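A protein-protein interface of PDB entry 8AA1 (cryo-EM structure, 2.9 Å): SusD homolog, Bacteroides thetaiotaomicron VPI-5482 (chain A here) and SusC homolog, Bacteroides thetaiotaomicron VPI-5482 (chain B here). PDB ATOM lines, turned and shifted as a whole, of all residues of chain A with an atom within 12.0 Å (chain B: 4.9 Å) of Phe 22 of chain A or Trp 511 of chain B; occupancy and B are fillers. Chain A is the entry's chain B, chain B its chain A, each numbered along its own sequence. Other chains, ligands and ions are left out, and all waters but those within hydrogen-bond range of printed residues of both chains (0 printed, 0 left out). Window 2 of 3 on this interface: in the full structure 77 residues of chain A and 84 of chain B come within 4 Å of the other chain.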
ATOM      1  N   ASP A  20      28.490  -6.063  13.310  1.00  0.00           N
ATOM      2  CA  ASP A  20      27.237  -5.693  13.957  1.00  0.00           C
ATOM      3  C   ASP A  20      26.209  -5.243  12.924  1.00  0.00           C
ATOM      4  O   ASP A  20      26.254  -4.113  12.439  1.00  0.00           O
ATOM      5  CB  ASP A  20      27.473  -4.586  14.987  1.00  0.00           C
ATOM      6  CG  ASP A  20      26.291  -4.395  15.918  1.00  0.00           C
ATOM      7  OD1 ASP A  20      25.360  -5.227  15.880  1.00  0.00           O
ATOM      8  OD2 ASP A  20      26.293  -3.412  16.687  1.00  0.00           O
ATOM      9  N   ASP A  21      25.281  -6.138  12.594  1.00  0.00           N
ATOM     10  CA  ASP A  21      24.240  -5.862  11.614  1.00  0.00           C
ATOM     11  C   ASP A  21      22.988  -5.257  12.236  1.00  0.00           C
ATOM     12  O   ASP A  21      21.974  -5.116  11.545  1.00  0.00           O
ATOM     13  CB  ASP A  21      23.880  -7.142  10.856  1.00  0.00           C
ATOM     14  CG  ASP A  21      23.321  -8.218  11.764  1.00  0.00           C
ATOM     15  OD1 ASP A  21      23.729  -8.272  12.943  1.00  0.00           O
ATOM     16  OD2 ASP A  21      22.476  -9.011  11.298  1.00  0.00           O
ATOM     17  N   PHE A  22      23.034  -4.905  13.523  1.00  0.00           N
ATOM     18  CA  PHE A  22      21.876  -4.297  14.171  1.00  0.00           C
ATOM     19  C   PHE A  22      21.508  -2.967  13.528  1.00  0.00           C
ATOM     20  O   PHE A  22      20.325  -2.676  13.320  1.00  0.00           O
ATOM     21  CB  PHE A  22      22.148  -4.112  15.662  1.00  0.00           C
ATOM     22  CG  PHE A  22      20.918  -3.828  16.469  1.00  0.00           C
ATOM     23  CD1 PHE A  22      20.168  -4.856  17.010  1.00  0.00           C
ATOM     24  CD2 PHE A  22      20.516  -2.523  16.694  1.00  0.00           C
ATOM     25  CE1 PHE A  22      19.036  -4.587  17.755  1.00  0.00           C
ATOM     26  CE2 PHE A  22      19.388  -2.248  17.437  1.00  0.00           C
ATOM     27  CZ  PHE A  22      18.647  -3.280  17.968  1.00  0.00           C
ATOM     28  N   LEU A  23      22.502  -2.150  13.203  1.00  0.00           N
ATOM     29  CA  LEU A  23      22.261  -0.822  12.659  1.00  0.00           C
ATOM     30  C   LEU A  23      22.260  -0.792  11.136  1.00  0.00           C
ATOM     31  O   LEU A  23      22.223   0.297  10.555  1.00  0.00           O
ATOM     32  CB  LEU A  23      23.309   0.160  13.196  1.00  0.00           C
ATOM     33  CG  LEU A  23      23.338   0.343  14.716  1.00  0.00           C
ATOM     34  CD1 LEU A  23      24.575   1.104  15.155  1.00  0.00           C
ATOM     35  CD2 LEU A  23      22.086   1.063  15.180  1.00  0.00           C
ATOM     36  N   ASP A  24      22.304  -1.950  10.474  1.00  0.00           N
ATOM     37  CA  ASP A  24      22.493  -1.995   9.033  1.00  0.00           C
ATOM     38  C   ASP A  24      21.426  -2.762   8.263  1.00  0.00           C
ATOM     39  O   ASP A  24      21.478  -2.762   7.028  1.00  0.00           O
ATOM     40  CB  ASP A  24      23.868  -2.589   8.696  1.00  0.00           C
ATOM     41  CG  ASP A  24      25.012  -1.673   9.089  1.00  0.00           C
ATOM     42  OD1 ASP A  24      24.868  -0.444   8.936  1.00  0.00           O
ATOM     43  OD2 ASP A  24      26.066  -2.183   9.526  1.00  0.00           O
ATOM     44  N   ARG A  25      20.472  -3.426   8.925  1.00  0.00           N
ATOM     45  CA  ARG A  25      19.468  -4.139   8.141  1.00  0.00           C
ATOM     46  C   ARG A  25      18.625  -3.160   7.342  1.00  0.00           C
ATOM     47  O   ARG A  25      18.269  -3.426   6.189  1.00  0.00           O
ATOM     48  CB  ARG A  25      18.527  -4.973   9.013  1.00  0.00           C
ATOM     49  CG  ARG A  25      17.707  -4.186  10.028  1.00  0.00           C
ATOM     50  CD  ARG A  25      16.958  -5.108  10.970  1.00  0.00           C
ATOM     51  NE  ARG A  25      15.907  -4.407  11.696  1.00  0.00           N
ATOM     52  CZ  ARG A  25      14.902  -5.012  12.313  1.00  0.00           C
ATOM     53  NH1 ARG A  25      14.803  -6.331  12.342  1.00  0.00           N
ATOM     54  NH2 ARG A  25      13.964  -4.275  12.904  1.00  0.00           N
ATOM     55  N   GLN A  26      18.311  -2.016   7.942  1.00  0.00           N
ATOM     56  CA  GLN A  26      17.213  -1.175   7.506  1.00  0.00           C
ATOM     57  C   GLN A  26      17.631  -0.336   6.311  1.00  0.00           C
ATOM     58  O   GLN A  26      18.743   0.199   6.263  1.00  0.00           O
ATOM     59  CB  GLN A  26      16.751  -0.292   8.666  1.00  0.00           C
ATOM     60  CG  GLN A  26      15.867  -1.047   9.656  1.00  0.00           C
ATOM     61  CD  GLN A  26      15.345  -0.186  10.790  1.00  0.00           C
ATOM     62  OE1 GLN A  26      15.838   0.915  11.027  1.00  0.00           O
ATOM     63  NE2 GLN A  26      14.348  -0.692  11.504  1.00  0.00           N
ATOM     64  N   VAL A  27      16.731  -0.239   5.341  1.00  0.00           N
ATOM     65  CA  VAL A  27      17.010   0.438   4.077  1.00  0.00           C
ATOM     66  C   VAL A  27      15.883   1.421   3.813  1.00  0.00           C
ATOM     67  O   VAL A  27      14.798   1.322   4.408  1.00  0.00           O
ATOM     68  CB  VAL A  27      17.155  -0.568   2.911  1.00  0.00           C
ATOM     69  CG1 VAL A  27      18.422  -1.395   3.066  1.00  0.00           C
ATOM     70  CG2 VAL A  27      15.932  -1.455   2.833  1.00  0.00           C
ATOM     71  N   PHE B 472      13.522  -5.603  29.146  1.00  0.00           N
ATOM     72  CA  PHE B 472      12.936  -5.536  27.814  1.00  0.00           C
ATOM     73  C   PHE B 472      11.681  -4.681  27.887  1.00  0.00           C
ATOM     74  O   PHE B 472      10.734  -5.027  28.600  1.00  0.00           O
ATOM     75  CB  PHE B 472      12.608  -6.931  27.278  1.00  0.00           C
ATOM     76  CG  PHE B 472      12.149  -6.937  25.848  1.00  0.00           C
ATOM     77  CD1 PHE B 472      13.067  -6.949  24.813  1.00  0.00           C
ATOM     78  CD2 PHE B 472      10.800  -6.934  25.540  1.00  0.00           C
ATOM     79  CE1 PHE B 472      12.648  -6.954  23.497  1.00  0.00           C
ATOM     80  CE2 PHE B 472      10.374  -6.940  24.226  1.00  0.00           C
ATOM     81  CZ  PHE B 472      11.300  -6.950  23.204  1.00  0.00           C
ATOM     82  N   GLY B 473      11.676  -3.579  27.154  1.00  0.00           N
ATOM     83  CA  GLY B 473      10.543  -2.665  27.131  1.00  0.00           C
ATOM     84  C   GLY B 473       9.956  -2.575  25.737  1.00  0.00           C
ATOM     85  O   GLY B 473      10.688  -2.604  24.747  1.00  0.00           O
ATOM     86  N   LEU B 474       8.633  -2.460  25.670  1.00  0.00           N
ATOM     87  CA  LEU B 474       7.892  -2.430  24.419  1.00  0.00           C
ATOM     88  C   LEU B 474       6.900  -1.276  24.435  1.00  0.00           C
ATOM     89  O   LEU B 474       6.282  -0.990  25.464  1.00  0.00           O
ATOM     90  CB  LEU B 474       7.152  -3.754  24.190  1.00  0.00           C
ATOM     91  CG  LEU B 474       6.262  -3.862  22.951  1.00  0.00           C
ATOM     92  CD1 LEU B 474       7.094  -3.760  21.686  1.00  0.00           C
ATOM     93  CD2 LEU B 474       5.472  -5.159  22.975  1.00  0.00           C
ATOM     94  N   THR B 509       5.944   0.757  16.541  1.00  0.00           N
ATOM     95  CA  THR B 509       6.413  -0.362  17.354  1.00  0.00           C
ATOM     96  C   THR B 509       7.861  -0.095  17.736  1.00  0.00           C
ATOM     97  O   THR B 509       8.745  -0.126  16.877  1.00  0.00           O
ATOM     98  CB  THR B 509       6.285  -1.687  16.604  1.00  0.00           C
ATOM     99  OG1 THR B 509       4.918  -1.897  16.229  1.00  0.00           O
ATOM    100  CG2 THR B 509       6.746  -2.841  17.480  1.00  0.00           C
ATOM    101  N   LYS B 510       8.103   0.169  19.016  1.00  0.00           N
ATOM    102  CA  LYS B 510       9.445   0.403  19.529  1.00  0.00           C
ATOM    103  C   LYS B 510       9.744  -0.630  20.604  1.00  0.00           C
ATOM    104  O   LYS B 510       8.865  -0.979  21.393  1.00  0.00           O
ATOM    105  CB  LYS B 510       9.585   1.817  20.098  1.00  0.00           C
ATOM    106  CG  LYS B 510       8.651   2.837  19.470  1.00  0.00           C
ATOM    107  CD  LYS B 510       8.806   4.199  20.124  1.00  0.00           C
ATOM    108  CE  LYS B 510       7.640   5.112  19.784  1.00  0.00           C
ATOM    109  NZ  LYS B 510       7.457   5.249  18.314  1.00  0.00           N
ATOM    110  N   TRP B 511      10.971  -1.136  20.619  1.00  0.00           N
ATOM    111  CA  TRP B 511      11.387  -2.022  21.694  1.00  0.00           C
ATOM    112  C   TRP B 511      12.834  -1.746  22.067  1.00  0.00           C
ATOM    113  O   TRP B 511      13.663  -1.418  21.212  1.00  0.00           O
ATOM    114  CB  TRP B 511      11.190  -3.503  21.330  1.00  0.00           C
ATOM    115  CG  TRP B 511      12.069  -4.030  20.243  1.00  0.00           C
ATOM    116  CD1 TRP B 511      11.739  -4.189  18.931  1.00  0.00           C
ATOM    117  CD2 TRP B 511      13.414  -4.506  20.379  1.00  0.00           C
ATOM    118  NE1 TRP B 511      12.796  -4.723  18.238  1.00  0.00           N
ATOM    119  CE2 TRP B 511      13.838  -4.923  19.104  1.00  0.00           C
ATOM    120  CE3 TRP B 511      14.302  -4.613  21.454  1.00  0.00           C
ATOM    121  CZ2 TRP B 511      15.111  -5.436  18.872  1.00  0.00           C
ATOM    122  CZ3 TRP B 511      15.564  -5.122  21.221  1.00  0.00           C
ATOM    123  CH2 TRP B 511      15.957  -5.527  19.942  1.00  0.00           C
ATOM    124  N   MET B 512      13.119  -1.873  23.359  1.00  0.00           N
ATOM    125  CA  MET B 512      14.439  -1.623  23.914  1.00  0.00           C
ATOM    126  C   MET B 512      14.866  -2.803  24.771  1.00  0.00           C
ATOM    127  O   MET B 512      14.078  -3.327  25.564  1.00  0.00           O
ATOM    128  CB  MET B 512      14.456  -0.334  24.747  1.00  0.00           C
ATOM    129  CG  MET B 512      15.587  -0.259  25.761  1.00  0.00           C
ATOM    130  SD  MET B 512      15.049   0.311  27.384  1.00  0.00           S
ATOM    131  CE  MET B 512      14.620  -1.239  28.170  1.00  0.00           C
ATOM    132  N   TRP B 513      16.118  -3.214  24.607  1.00  0.00           N
ATOM    133  CA  TRP B 513      16.743  -4.224  25.448  1.00  0.00           C
ATOM    134  C   TRP B 513      17.914  -3.594  26.186  1.00  0.00           C
ATOM    135  O   TRP B 513      18.707  -2.858  25.595  1.00  0.00           O
ATOM    136  CB  TRP B 513      17.221  -5.423  24.627  1.00  0.00           C
ATOM    137  CG  TRP B 513      17.860  -6.489  25.457  1.00  0.00           C
ATOM    138  CD1 TRP B 513      17.226  -7.422  26.223  1.00  0.00           C
ATOM    139  CD2 TRP B 513      19.264  -6.729  25.612  1.00  0.00           C
ATOM    140  NE1 TRP B 513      18.146  -8.231  26.843  1.00  0.00           N
ATOM    141  CE2 TRP B 513      19.405  -7.826  26.484  1.00  0.00           C
ATOM    142  CE3 TRP B 513      20.414  -6.125  25.097  1.00  0.00           C
ATOM    143  CZ2 TRP B 513      20.649  -8.331  26.852  1.00  0.00           C
ATOM    144  CZ3 TRP B 513      21.647  -6.627  25.463  1.00  0.00           C
ATOM    145  CH2 TRP B 513      21.756  -7.719  26.332  1.00  0.00           C
ATOM    146  N   LEU B 536      20.012  -1.399  23.485  1.00  0.00           N
ATOM    147  CA  LEU B 536      19.572  -1.394  22.098  1.00  0.00           C
ATOM    148  C   LEU B 536      18.156  -0.846  22.036  1.00  0.00           C
ATOM    149  O   LEU B 536      17.277  -1.307  22.770  1.00  0.00           O
ATOM    150  CB  LEU B 536      19.618  -2.798  21.493  1.00  0.00           C
ATOM    151  CG  LEU B 536      20.935  -3.569  21.594  1.00  0.00           C
ATOM    152  CD1 LEU B 536      20.777  -4.962  21.013  1.00  0.00           C
ATOM    153  CD2 LEU B 536      22.053  -2.824  20.890  1.00  0.00           C
ATOM    154  N   ASN B 537      17.938   0.126  21.158  1.00  0.00           N
ATOM    155  CA  ASN B 537      16.621   0.704  20.940  1.00  0.00           C
ATOM    156  C   ASN B 537      16.270   0.524  19.476  1.00  0.00           C
ATOM    157  O   ASN B 537      17.132   0.668  18.609  1.00  0.00           O
ATOM    158  CB  ASN B 537      16.587   2.186  21.313  1.00  0.00           C
ATOM    159  CG  ASN B 537      16.803   2.417  22.791  1.00  0.00           C
ATOM    160  OD1 ASN B 537      15.858   2.649  23.540  1.00  0.00           O
ATOM    161  ND2 ASN B 537      18.058   2.351  23.219  1.00  0.00           N
ATOM    162  N   ARG B 538      15.014   0.200  19.190  1.00  0.00           N
ATOM    163  CA  ARG B 538      14.658  -0.248  17.851  1.00  0.00           C
ATOM    164  C   ARG B 538      13.229   0.182  17.562  1.00  0.00           C
ATOM    165  O   ARG B 538      12.298  -0.334  18.184  1.00  0.00           O
ATOM    166  CB  ARG B 538      14.798  -1.772  17.782  1.00  0.00           C
ATOM    167  CG  ARG B 538      14.164  -2.460  16.606  1.00  0.00           C
ATOM    168  CD  ARG B 538      14.689  -1.943  15.289  1.00  0.00           C
ATOM    169  NE  ARG B 538      16.051  -2.408  15.027  1.00  0.00           N
ATOM    170  CZ  ARG B 538      16.421  -3.680  14.924  1.00  0.00           C
ATOM    171  NH1 ARG B 538      15.570  -4.676  15.129  1.00  0.00           N
ATOM    172  NH2 ARG B 538      17.685  -3.965  14.623  1.00  0.00           N
ATOM    173  N   SER B 578      17.432   2.489  14.537  1.00  0.00           N
ATOM    174  CA  SER B 578      17.972   1.715  15.643  1.00  0.00           C
ATOM    175  C   SER B 578      19.086   2.501  16.319  1.00  0.00           C
ATOM    176  O   SER B 578      19.742   3.341  15.700  1.00  0.00           O
ATOM    177  CB  SER B 578      18.500   0.354  15.173  1.00  0.00           C
ATOM    178  OG  SER B 578      17.473  -0.410  14.569  1.00  0.00           O
ATOM    179  N   LEU B 579      19.289   2.212  17.602  1.00  0.00           N
ATOM    180  CA  LEU B 579      20.294   2.866  18.425  1.00  0.00           C
ATOM    181  C   LEU B 579      21.018   1.816  19.251  1.00  0.00           C
ATOM    182  O   LEU B 579      20.387   0.904  19.794  1.00  0.00           O
ATOM    183  CB  LEU B 579      19.663   3.906  19.360  1.00  0.00           C
ATOM    184  CG  LEU B 579      18.724   4.951  18.760  1.00  0.00           C
ATOM    185  CD1 LEU B 579      18.019   5.714  19.866  1.00  0.00           C
ATOM    186  CD2 LEU B 579      19.482   5.904  17.859  1.00  0.00           C
ATOM    187  N   VAL B 580      22.336   1.962  19.360  1.00  0.00           N
ATOM    188  CA  VAL B 580      23.176   1.088  20.170  1.00  0.00           C
ATOM    189  C   VAL B 580      23.972   1.964  21.125  1.00  0.00           C
ATOM    190  O   VAL B 580      24.512   2.998  20.718  1.00  0.00           O
ATOM    191  CB  VAL B 580      24.123   0.235  19.303  1.00  0.00           C
ATOM    192  CG1 VAL B 580      24.987  -0.658  20.178  1.00  0.00           C
ATOM    193  CG2 VAL B 580      23.334  -0.593  18.305  1.00  0.00           C
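O of Phe 22 of chain A is in hydrogen-bond range of NH2 of Arg 538 of chain B (3.2 Å). The guanidinium group (NH1) of Arg 538 of chain B sits close to the guanidinium group (NH2) of Arg 25 of chain A.
NE of Arg 538 of chain B sits at hydrogen-bond distance from OG of Ser 578 of chain B, at 2.5 Å. The backbone NH of Leu 579 of chain B sits at hydrogen-bond distance from the backbone carbonyl oxygen of Asn 537 of chain B. N of Trp 511 of chain B is in hydrogen-bond range of O of Arg 538 of chain B (2.9 Å). O of Trp 513 of chain B sits at hydrogen-bond distance from N of Leu 536 of chain B (2.9 Å). The side-chain carboxylate of Asp 20 of chain A sits close to the backbone NH of Phe 22 of chain A (3.3 Å).
Among the printed residues, pairs that only touch across the chains: Phe 22 of chain A with Trp 511 of chain B (3.9 Å), Phe 22 of chain A with Leu 536 of chain B (3.7 Å), Phe 22 of chain A with Asn 537 of chain B (3.9 Å), Phe 22 of chain A with Ser 578 of chain B (3.6 Å), Phe 22 of chain A with Val 580 of chain B (3.8 Å), Leu 23 of chain A with Ser 578 of chain B (3.3 Å), Leu 23 of chain A with Leu 579 of chain B (3.9 Å) and Leu 23 of chain A with Val 580 of chain B (3.7 Å).
Asp 20 of chain A touches none of the printed residues of chain B. Of chain B, only Trp 511 (3.9 Å), Leu 536 (3.7 Å), Asn 537 (3.9 Å), Arg 538 (3.2 Å), Ser 578 (3.6 Å) and Val 580 (3.8 Å) come within 4 Å of Phe 22 of chain A. Of the printed residues of chain B, Leu 23 of chain A touches Ser 578 (3.3 Å), Leu 579 (3.9 Å) and Val 580 (3.7 Å). Val 27 of chain A touches none of the printed residues of chain B. Phe 472 of chain B touches none of the printed residues of chain A. No residue of chain A comes within 4 Å of Leu 474 of chain B. No residue of chain A comes within 4 Å of Thr 509 of chain B. Of chain A, only Phe 22 comes within 4 Å of Leu 536 of chain B. Of chain A, only Phe 22 (3.9 Å) comes within 4 Å of Asn 537 of chain B. Ser 578 of chain B touches two residues of chain A. Printed residues of chain A within 4 Å of Leu 579 of chain B: Leu 23 (3.9 Å). Val 580 of chain B touches two residues of chain A.
Of the 14 printed residues of chain B, 7 touch a printed residue of chain A. Hydrophobic or aromatic side chains of chain B within 4 Å of the printed part of chain A: Trp 511, Leu 536 and Val 580. Printed residues of chain A that touch a printed residue of chain B: Phe 22, Leu 23 and Arg 25. Hydrophobic or aromatic side chains of chain A that line the printed part of chain B: Phe 22 and Leu 23. Along chain A the printed residues that touch a printed residue of chain B span positions 22 to 25. Among the printed residues, 10 pairs touch across the chains. Among the printed residues, no Asp or Glu carboxylate lies within 4 Å of a Lys or Arg side-chain nitrogen of the other chain.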
